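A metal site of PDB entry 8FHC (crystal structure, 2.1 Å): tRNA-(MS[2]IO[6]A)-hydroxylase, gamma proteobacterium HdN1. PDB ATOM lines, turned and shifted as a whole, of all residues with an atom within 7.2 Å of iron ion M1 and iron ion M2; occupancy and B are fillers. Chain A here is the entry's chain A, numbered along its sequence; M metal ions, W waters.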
ATOM      1  N   HIS A  42      -0.736 -19.317 -21.830  1.00  0.00           N
ATOM      2  CA  HIS A  42      -1.720 -18.262 -21.683  1.00  0.00           C
ATOM      3  C   HIS A  42      -1.687 -17.374 -22.925  1.00  0.00           C
ATOM      4  O   HIS A  42      -2.697 -17.227 -23.602  1.00  0.00           O
ATOM      5  CB  HIS A  42      -1.510 -17.520 -20.348  1.00  0.00           C
ATOM      6  CG  HIS A  42      -2.433 -16.383 -20.119  1.00  0.00           C
ATOM      7  ND1 HIS A  42      -2.293 -15.611 -18.992  1.00  0.00           N
ATOM      8  CD2 HIS A  42      -3.451 -15.850 -20.807  1.00  0.00           C
ATOM      9  CE1 HIS A  42      -3.193 -14.634 -19.020  1.00  0.00           C
ATOM     10  NE2 HIS A  42      -3.895 -14.740 -20.119  1.00  0.00           N
ATOM     11  N   CYS A  45      -3.377 -19.053 -25.726  1.00  0.00           N
ATOM     12  CA  CYS A  45      -4.808 -19.144 -25.562  1.00  0.00           C
ATOM     13  C   CYS A  45      -5.514 -17.861 -25.965  1.00  0.00           C
ATOM     14  O   CYS A  45      -6.615 -17.928 -26.468  1.00  0.00           O
ATOM     15  CB  CYS A  45      -5.189 -19.441 -24.112  1.00  0.00           C
ATOM     16  SG  CYS A  45      -4.839 -21.158 -23.706  1.00  0.00           S
ATOM     17  N   GLU A  46      -4.913 -16.710 -25.646  1.00  0.00           N
ATOM     18  CA  GLU A  46      -5.474 -15.429 -25.996  1.00  0.00           C
ATOM     19  C   GLU A  46      -5.541 -15.276 -27.522  1.00  0.00           C
ATOM     20  O   GLU A  46      -6.534 -14.787 -28.047  1.00  0.00           O
ATOM     21  CB  GLU A  46      -4.650 -14.297 -25.410  1.00  0.00           C
ATOM     22  CG  GLU A  46      -4.525 -14.323 -23.907  1.00  0.00           C
ATOM     23  CD  GLU A  46      -5.781 -13.952 -23.128  1.00  0.00           C
ATOM     24  OE1 GLU A  46      -5.706 -13.877 -21.892  1.00  0.00           O
ATOM     25  OE2 GLU A  46      -6.792 -13.638 -23.767  1.00  0.00           O
ATOM     26  N   ALA A  49      -8.391 -17.453 -28.762  1.00  0.00           N
ATOM     27  CA  ALA A  49      -9.702 -16.883 -28.544  1.00  0.00           C
ATOM     28  C   ALA A  49      -9.962 -15.814 -29.617  1.00  0.00           C
ATOM     29  O   ALA A  49     -11.051 -15.720 -30.174  1.00  0.00           O
ATOM     30  CB  ALA A  49      -9.793 -16.375 -27.130  1.00  0.00           C
ATOM     31  N   LEU A  73     -14.819  -8.569 -28.869  1.00  0.00           N
ATOM     32  CA  LEU A  73     -14.147  -9.612 -28.124  1.00  0.00           C
ATOM     33  C   LEU A  73     -12.756  -9.915 -28.706  1.00  0.00           C
ATOM     34  O   LEU A  73     -11.786 -10.008 -27.958  1.00  0.00           O
ATOM     35  CB  LEU A  73     -15.060 -10.831 -28.118  1.00  0.00           C
ATOM     36  CG  LEU A  73     -14.773 -11.858 -27.015  1.00  0.00           C
ATOM     37  CD1 LEU A  73     -16.085 -12.386 -26.434  1.00  0.00           C
ATOM     38  CD2 LEU A  73     -13.916 -12.998 -27.558  1.00  0.00           C
ATOM     39  N   GLU A  76     -10.214  -7.400 -27.791  1.00  0.00           N
ATOM     40  CA  GLU A  76      -9.834  -7.490 -26.391  1.00  0.00           C
ATOM     41  C   GLU A  76      -8.874  -8.660 -26.187  1.00  0.00           C
ATOM     42  O   GLU A  76      -7.909  -8.556 -25.435  1.00  0.00           O
ATOM     43  CB  GLU A  76     -11.052  -7.631 -25.479  1.00  0.00           C
ATOM     44  CG  GLU A  76     -12.006  -6.465 -25.583  1.00  0.00           C
ATOM     45  CD  GLU A  76     -13.254  -6.507 -24.727  1.00  0.00           C
ATOM     46  OE1 GLU A  76     -13.365  -7.394 -23.846  1.00  0.00           O
ATOM     47  OE2 GLU A  76     -14.111  -5.626 -24.927  1.00  0.00           O
ATOM     48  N   GLU A  77      -9.105  -9.771 -26.889  1.00  0.00           N
ATOM     49  CA  GLU A  77      -8.249 -10.940 -26.732  1.00  0.00           C
ATOM     50  C   GLU A  77      -6.841 -10.646 -27.256  1.00  0.00           C
ATOM     51  O   GLU A  77      -5.852 -11.124 -26.704  1.00  0.00           O
ATOM     52  CB  GLU A  77      -8.802 -12.155 -27.465  1.00  0.00           C
ATOM     53  CG  GLU A  77     -10.173 -12.614 -27.020  1.00  0.00           C
ATOM     54  CD  GLU A  77     -10.274 -13.090 -25.578  1.00  0.00           C
ATOM     55  OE1 GLU A  77     -11.364 -13.505 -25.179  1.00  0.00           O
ATOM     56  OE2 GLU A  77      -9.286 -13.007 -24.846  1.00  0.00           O
ATOM     57  N   LEU A  78      -6.741  -9.855 -28.350  1.00  0.00           N
ATOM     58  CA  LEU A  78      -5.453  -9.501 -28.937  1.00  0.00           C
ATOM     59  C   LEU A  78      -4.708  -8.583 -27.987  1.00  0.00           C
ATOM     60  O   LEU A  78      -3.483  -8.611 -27.931  1.00  0.00           O
ATOM     61  CB  LEU A  78      -5.672  -8.833 -30.295  1.00  0.00           C
ATOM     62  CG  LEU A  78      -6.027  -9.789 -31.439  1.00  0.00           C
ATOM     63  CD1 LEU A  78      -6.473  -9.045 -32.685  1.00  0.00           C
ATOM     64  CD2 LEU A  78      -4.845 -10.719 -31.743  1.00  0.00           C
ATOM     65  N   LEU A  79      -5.444  -7.734 -27.284  1.00  0.00           N
ATOM     66  CA  LEU A  79      -4.900  -6.839 -26.275  1.00  0.00           C
ATOM     67  C   LEU A  79      -4.374  -7.699 -25.112  1.00  0.00           C
ATOM     68  O   LEU A  79      -3.265  -7.483 -24.638  1.00  0.00           O
ATOM     69  CB  LEU A  79      -6.040  -5.915 -25.843  1.00  0.00           C
ATOM     70  CG  LEU A  79      -5.739  -4.447 -25.554  1.00  0.00           C
ATOM     71  CD1 LEU A  79      -5.066  -3.754 -26.716  1.00  0.00           C
ATOM     72  CD2 LEU A  79      -7.055  -3.729 -25.267  1.00  0.00           C
ATOM     73  N   HIS A  80      -5.175  -8.679 -24.655  1.00  0.00           N
ATOM     74  CA  HIS A  80      -4.687  -9.629 -23.667  1.00  0.00           C
ATOM     75  C   HIS A  80      -3.372 -10.258 -24.134  1.00  0.00           C
ATOM     76  O   HIS A  80      -2.449 -10.384 -23.345  1.00  0.00           O
ATOM     77  CB  HIS A  80      -5.753 -10.685 -23.346  1.00  0.00           C
ATOM     78  CG  HIS A  80      -6.956 -10.104 -22.680  1.00  0.00           C
ATOM     79  ND1 HIS A  80      -8.142 -10.788 -22.509  1.00  0.00           N
ATOM     80  CD2 HIS A  80      -7.111  -8.907 -22.088  1.00  0.00           C
ATOM     81  CE1 HIS A  80      -8.991 -10.013 -21.877  1.00  0.00           C
ATOM     82  NE2 HIS A  80      -8.366  -8.865 -21.586  1.00  0.00           N
ATOM     83  N   PHE A  81      -3.298 -10.632 -25.409  1.00  0.00           N
ATOM     84  CA  PHE A  81      -2.102 -11.266 -25.967  1.00  0.00           C
ATOM     85  C   PHE A  81      -0.880 -10.357 -25.790  1.00  0.00           C
ATOM     86  O   PHE A  81       0.146 -10.788 -25.275  1.00  0.00           O
ATOM     87  CB  PHE A  81      -2.271 -11.635 -27.440  1.00  0.00           C
ATOM     88  CG  PHE A  81      -1.001 -12.077 -28.123  1.00  0.00           C
ATOM     89  CD1 PHE A  81      -0.358 -13.249 -27.753  1.00  0.00           C
ATOM     90  CD2 PHE A  81      -0.394 -11.290 -29.092  1.00  0.00           C
ATOM     91  CE1 PHE A  81       0.831 -13.641 -28.358  1.00  0.00           C
ATOM     92  CE2 PHE A  81       0.812 -11.662 -29.671  1.00  0.00           C
ATOM     93  CZ  PHE A  81       1.407 -12.849 -29.322  1.00  0.00           C
ATOM     94  N   ILE A 129     -15.143 -22.203 -22.281  1.00  0.00           N
ATOM     95  CA  ILE A 129     -13.733 -21.847 -22.251  1.00  0.00           C
ATOM     96  C   ILE A 129     -13.553 -20.559 -21.445  1.00  0.00           C
ATOM     97  O   ILE A 129     -12.624 -20.457 -20.653  1.00  0.00           O
ATOM     98  CB  ILE A 129     -13.160 -21.735 -23.664  1.00  0.00           C
ATOM     99  CG1 ILE A 129     -13.146 -23.093 -24.360  1.00  0.00           C
ATOM    100  CG2 ILE A 129     -11.771 -21.122 -23.647  1.00  0.00           C
ATOM    101  CD1 ILE A 129     -12.684 -23.019 -25.782  1.00  0.00           C
ATOM    102  N   GLU A 130     -14.436 -19.583 -21.656  1.00  0.00           N
ATOM    103  CA  GLU A 130     -14.259 -18.272 -21.034  1.00  0.00           C
ATOM    104  C   GLU A 130     -14.600 -18.393 -19.543  1.00  0.00           C
ATOM    105  O   GLU A 130     -13.898 -17.829 -18.702  1.00  0.00           O
ATOM    106  CB  GLU A 130     -15.128 -17.229 -21.741  1.00  0.00           C
ATOM    107  CG  GLU A 130     -14.728 -16.897 -23.182  1.00  0.00           C
ATOM    108  CD  GLU A 130     -13.347 -16.290 -23.393  1.00  0.00           C
ATOM    109  OE1 GLU A 130     -13.267 -15.097 -23.718  1.00  0.00           O
ATOM    110  OE2 GLU A 130     -12.340 -17.004 -23.286  1.00  0.00           O
ATOM    111  N   SER A 133     -11.569 -20.230 -17.853  1.00  0.00           N
ATOM    112  CA  SER A 133     -10.455 -19.322 -17.702  1.00  0.00           C
ATOM    113  C   SER A 133     -10.695 -18.391 -16.507  1.00  0.00           C
ATOM    114  O   SER A 133      -9.782 -18.150 -15.721  1.00  0.00           O
ATOM    115  CB  SER A 133     -10.197 -18.533 -18.981  1.00  0.00           C
ATOM    116  OG  SER A 133      -9.971 -19.421 -20.076  1.00  0.00           O
ATOM    117  N   PHE A 137      -8.209 -18.293 -13.429  1.00  0.00           N
ATOM    118  CA  PHE A 137      -7.537 -17.069 -13.021  1.00  0.00           C
ATOM    119  C   PHE A 137      -7.891 -16.752 -11.574  1.00  0.00           C
ATOM    120  O   PHE A 137      -7.045 -16.264 -10.835  1.00  0.00           O
ATOM    121  CB  PHE A 137      -7.891 -15.877 -13.918  1.00  0.00           C
ATOM    122  CG  PHE A 137      -7.439 -15.918 -15.359  1.00  0.00           C
ATOM    123  CD1 PHE A 137      -6.145 -16.281 -15.710  1.00  0.00           C
ATOM    124  CD2 PHE A 137      -8.291 -15.525 -16.381  1.00  0.00           C
ATOM    125  CE1 PHE A 137      -5.739 -16.285 -17.042  1.00  0.00           C
ATOM    126  CE2 PHE A 137      -7.887 -15.547 -17.705  1.00  0.00           C
ATOM    127  CZ  PHE A 137      -6.616 -15.942 -18.035  1.00  0.00           C
ATOM    128  N   TYR A 156      -2.710  -8.906 -12.386  1.00  0.00           N
ATOM    129  CA  TYR A 156      -3.201  -9.009 -13.752  1.00  0.00           C
ATOM    130  C   TYR A 156      -4.310 -10.062 -13.832  1.00  0.00           C
ATOM    131  O   TYR A 156      -5.295  -9.847 -14.524  1.00  0.00           O
ATOM    132  CB  TYR A 156      -2.051  -9.331 -14.698  1.00  0.00           C
ATOM    133  CG  TYR A 156      -2.469  -9.398 -16.146  1.00  0.00           C
ATOM    134  CD1 TYR A 156      -3.164  -8.366 -16.738  1.00  0.00           C
ATOM    135  CD2 TYR A 156      -2.132 -10.494 -16.931  1.00  0.00           C
ATOM    136  CE1 TYR A 156      -3.537  -8.424 -18.075  1.00  0.00           C
ATOM    137  CE2 TYR A 156      -2.507 -10.571 -18.260  1.00  0.00           C
ATOM    138  CZ  TYR A 156      -3.213  -9.535 -18.844  1.00  0.00           C
ATOM    139  OH  TYR A 156      -3.556  -9.628 -20.183  1.00  0.00           O
ATOM    140  N   LEU A 160      -8.210  -9.559 -15.069  1.00  0.00           N
ATOM    141  CA  LEU A 160      -8.814 -10.269 -16.196  1.00  0.00           C
ATOM    142  C   LEU A 160     -10.208 -10.812 -15.882  1.00  0.00           C
ATOM    143  O   LEU A 160     -10.940 -11.153 -16.821  1.00  0.00           O
ATOM    144  CB  LEU A 160      -7.902 -11.423 -16.628  1.00  0.00           C
ATOM    145  CG  LEU A 160      -7.066 -11.232 -17.896  1.00  0.00           C
ATOM    146  CD1 LEU A 160      -6.846  -9.776 -18.236  1.00  0.00           C
ATOM    147  CD2 LEU A 160      -5.739 -11.954 -17.765  1.00  0.00           C
ATOM    148  N   SER A 163     -13.266  -9.148 -17.416  1.00  0.00           N
ATOM    149  CA  SER A 163     -13.195  -9.394 -18.855  1.00  0.00           C
ATOM    150  C   SER A 163     -13.785 -10.748 -19.219  1.00  0.00           C
ATOM    151  O   SER A 163     -14.677 -10.848 -20.051  1.00  0.00           O
ATOM    152  CB  SER A 163     -11.736  -9.315 -19.282  1.00  0.00           C
ATOM    153  OG  SER A 163     -11.629  -9.076 -20.668  1.00  0.00           O
ATOM    154  N   GLU A 164     -13.260 -11.786 -18.571  1.00  0.00           N
ATOM    155  CA  GLU A 164     -13.602 -13.160 -18.905  1.00  0.00           C
ATOM    156  C   GLU A 164     -15.063 -13.429 -18.572  1.00  0.00           C
ATOM    157  O   GLU A 164     -15.709 -14.202 -19.275  1.00  0.00           O
ATOM    158  CB  GLU A 164     -12.719 -14.149 -18.142  1.00  0.00           C
ATOM    159  CG  GLU A 164     -11.284 -14.142 -18.619  1.00  0.00           C
ATOM    160  CD  GLU A 164     -11.117 -14.591 -20.058  1.00  0.00           C
ATOM    161  OE1 GLU A 164     -12.136 -14.923 -20.689  1.00  0.00           O
ATOM    162  OE2 GLU A 164      -9.966 -14.606 -20.542  1.00  0.00           O
ATOM    163  N   SER A 165     -15.543 -12.835 -17.455  1.00  0.00           N
ATOM    164  CA  SER A 165     -16.915 -12.993 -17.016  1.00  0.00           C
ATOM    165  C   SER A 165     -17.868 -12.456 -18.079  1.00  0.00           C
ATOM    166  O   SER A 165     -18.866 -13.109 -18.431  1.00  0.00           O
ATOM    167  CB  SER A 165     -17.108 -12.301 -15.704  1.00  0.00           C
ATOM    168  OG  SER A 165     -18.459 -12.352 -15.317  1.00  0.00           O
ATOM    169  N   HIS A 167     -17.071 -12.039 -21.326  1.00  0.00           N
ATOM    170  CA  HIS A 167     -16.929 -12.864 -22.523  1.00  0.00           C
ATOM    171  C   HIS A 167     -17.815 -14.103 -22.429  1.00  0.00           C
ATOM    172  O   HIS A 167     -18.473 -14.484 -23.396  1.00  0.00           O
ATOM    173  CB  HIS A 167     -15.459 -13.229 -22.763  1.00  0.00           C
ATOM    174  CG  HIS A 167     -14.576 -12.078 -23.127  1.00  0.00           C
ATOM    175  ND1 HIS A 167     -13.211 -12.192 -23.224  1.00  0.00           N
ATOM    176  CD2 HIS A 167     -14.836 -10.789 -23.396  1.00  0.00           C
ATOM    177  CE1 HIS A 167     -12.665 -11.023 -23.564  1.00  0.00           C
ATOM    178  NE2 HIS A 167     -13.645 -10.164 -23.684  1.00  0.00           N
ATOM    179  N   PHE A 168     -17.821 -14.754 -21.261  1.00  0.00           N
ATOM    180  CA  PHE A 168     -18.660 -15.913 -20.986  1.00  0.00           C
ATOM    181  C   PHE A 168     -20.130 -15.552 -21.236  1.00  0.00           C
ATOM    182  O   PHE A 168     -20.859 -16.288 -21.921  1.00  0.00           O
ATOM    183  CB  PHE A 168     -18.438 -16.358 -19.535  1.00  0.00           C
ATOM    184  CG  PHE A 168     -19.633 -16.984 -18.876  1.00  0.00           C
ATOM    185  CD1 PHE A 168     -20.085 -18.240 -19.263  1.00  0.00           C
ATOM    186  CD2 PHE A 168     -20.326 -16.301 -17.879  1.00  0.00           C
ATOM    187  CE1 PHE A 168     -21.208 -18.799 -18.665  1.00  0.00           C
ATOM    188  CE2 PHE A 168     -21.447 -16.864 -17.291  1.00  0.00           C
ATOM    189  CZ  PHE A 168     -21.888 -18.101 -17.683  1.00  0.00           C
ATOM    190  N   TYR A 171     -20.898 -14.971 -25.024  1.00  0.00           N
ATOM    191  CA  TYR A 171     -20.974 -16.225 -25.777  1.00  0.00           C
ATOM    192  C   TYR A 171     -22.292 -16.926 -25.463  1.00  0.00           C
ATOM    193  O   TYR A 171     -23.000 -17.332 -26.371  1.00  0.00           O
ATOM    194  CB  TYR A 171     -19.729 -17.075 -25.526  1.00  0.00           C
ATOM    195  CG  TYR A 171     -18.643 -16.887 -26.563  1.00  0.00           C
ATOM    196  CD1 TYR A 171     -18.828 -17.318 -27.871  1.00  0.00           C
ATOM    197  CD2 TYR A 171     -17.421 -16.320 -26.243  1.00  0.00           C
ATOM    198  CE1 TYR A 171     -17.829 -17.215 -28.818  1.00  0.00           C
ATOM    199  CE2 TYR A 171     -16.420 -16.186 -27.192  1.00  0.00           C
ATOM    200  CZ  TYR A 171     -16.627 -16.622 -28.490  1.00  0.00           C
ATOM    201  OH  TYR A 171     -15.673 -16.472 -29.463  1.00  0.00           O
HETATM  202 FE    FE M   1     -11.746 -13.958 -23.128  1.00  0.00          FE
HETATM  203 FE    FE M   2      -8.598 -12.861 -22.881  1.00  0.00          FE
HETATM  204  O   HOH W   1      -9.636 -15.265 -23.073  1.00  0.00           O
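Water W1 bridges OE2 of Glu 164 (2.6 Å) and OE2 of Glu 130 (3.2 Å).
OE1 of Glu 130 binds iron ion M1, at 2.0 Å. Iron ion M1 is bound by OE1 of Glu 77 (2.1 Å). Iron ion M1 is bound by ND1 of His 167 (2.3 Å). Water W1 is bound to iron ion M1. Slightly farther from iron ion M1 lies the side-chain carboxylate (OE1) of Glu 164 (2.7 Å).
Within 4 Å of iron ion M1: Glu 77, Glu 130, Glu 164 and His 167. The nearest printed residue that does not touch iron ion M1 is His 80 (4.8 Å).
Iron ion M2 is bound by OE2 of Glu 77, ND1 of His 80 and OE2 of Glu 46. Slightly farther from iron ion M2 lies water W1 (2.6 Å).
The nearest printed residue that does not touch iron ion M2 is His 167 (4.5 Å).
The backbone carbonyl oxygen (O) of His 80 is in hydrogen-bond range of the side-chain hydroxyl (OH) of Tyr 156 (3.4 Å). A ring nitrogen (NE2) of His 167 is in hydrogen-bond range of the side-chain carboxylate of Glu 76, 2.8 Å away. A ring nitrogen (NE2) of His 42 sits at hydrogen-bond distance from the side-chain carboxylate (OE1) of Glu 46, at 2.7 Å. NE2 of His 80 lies close to OG of Ser 163 (3.4 Å).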
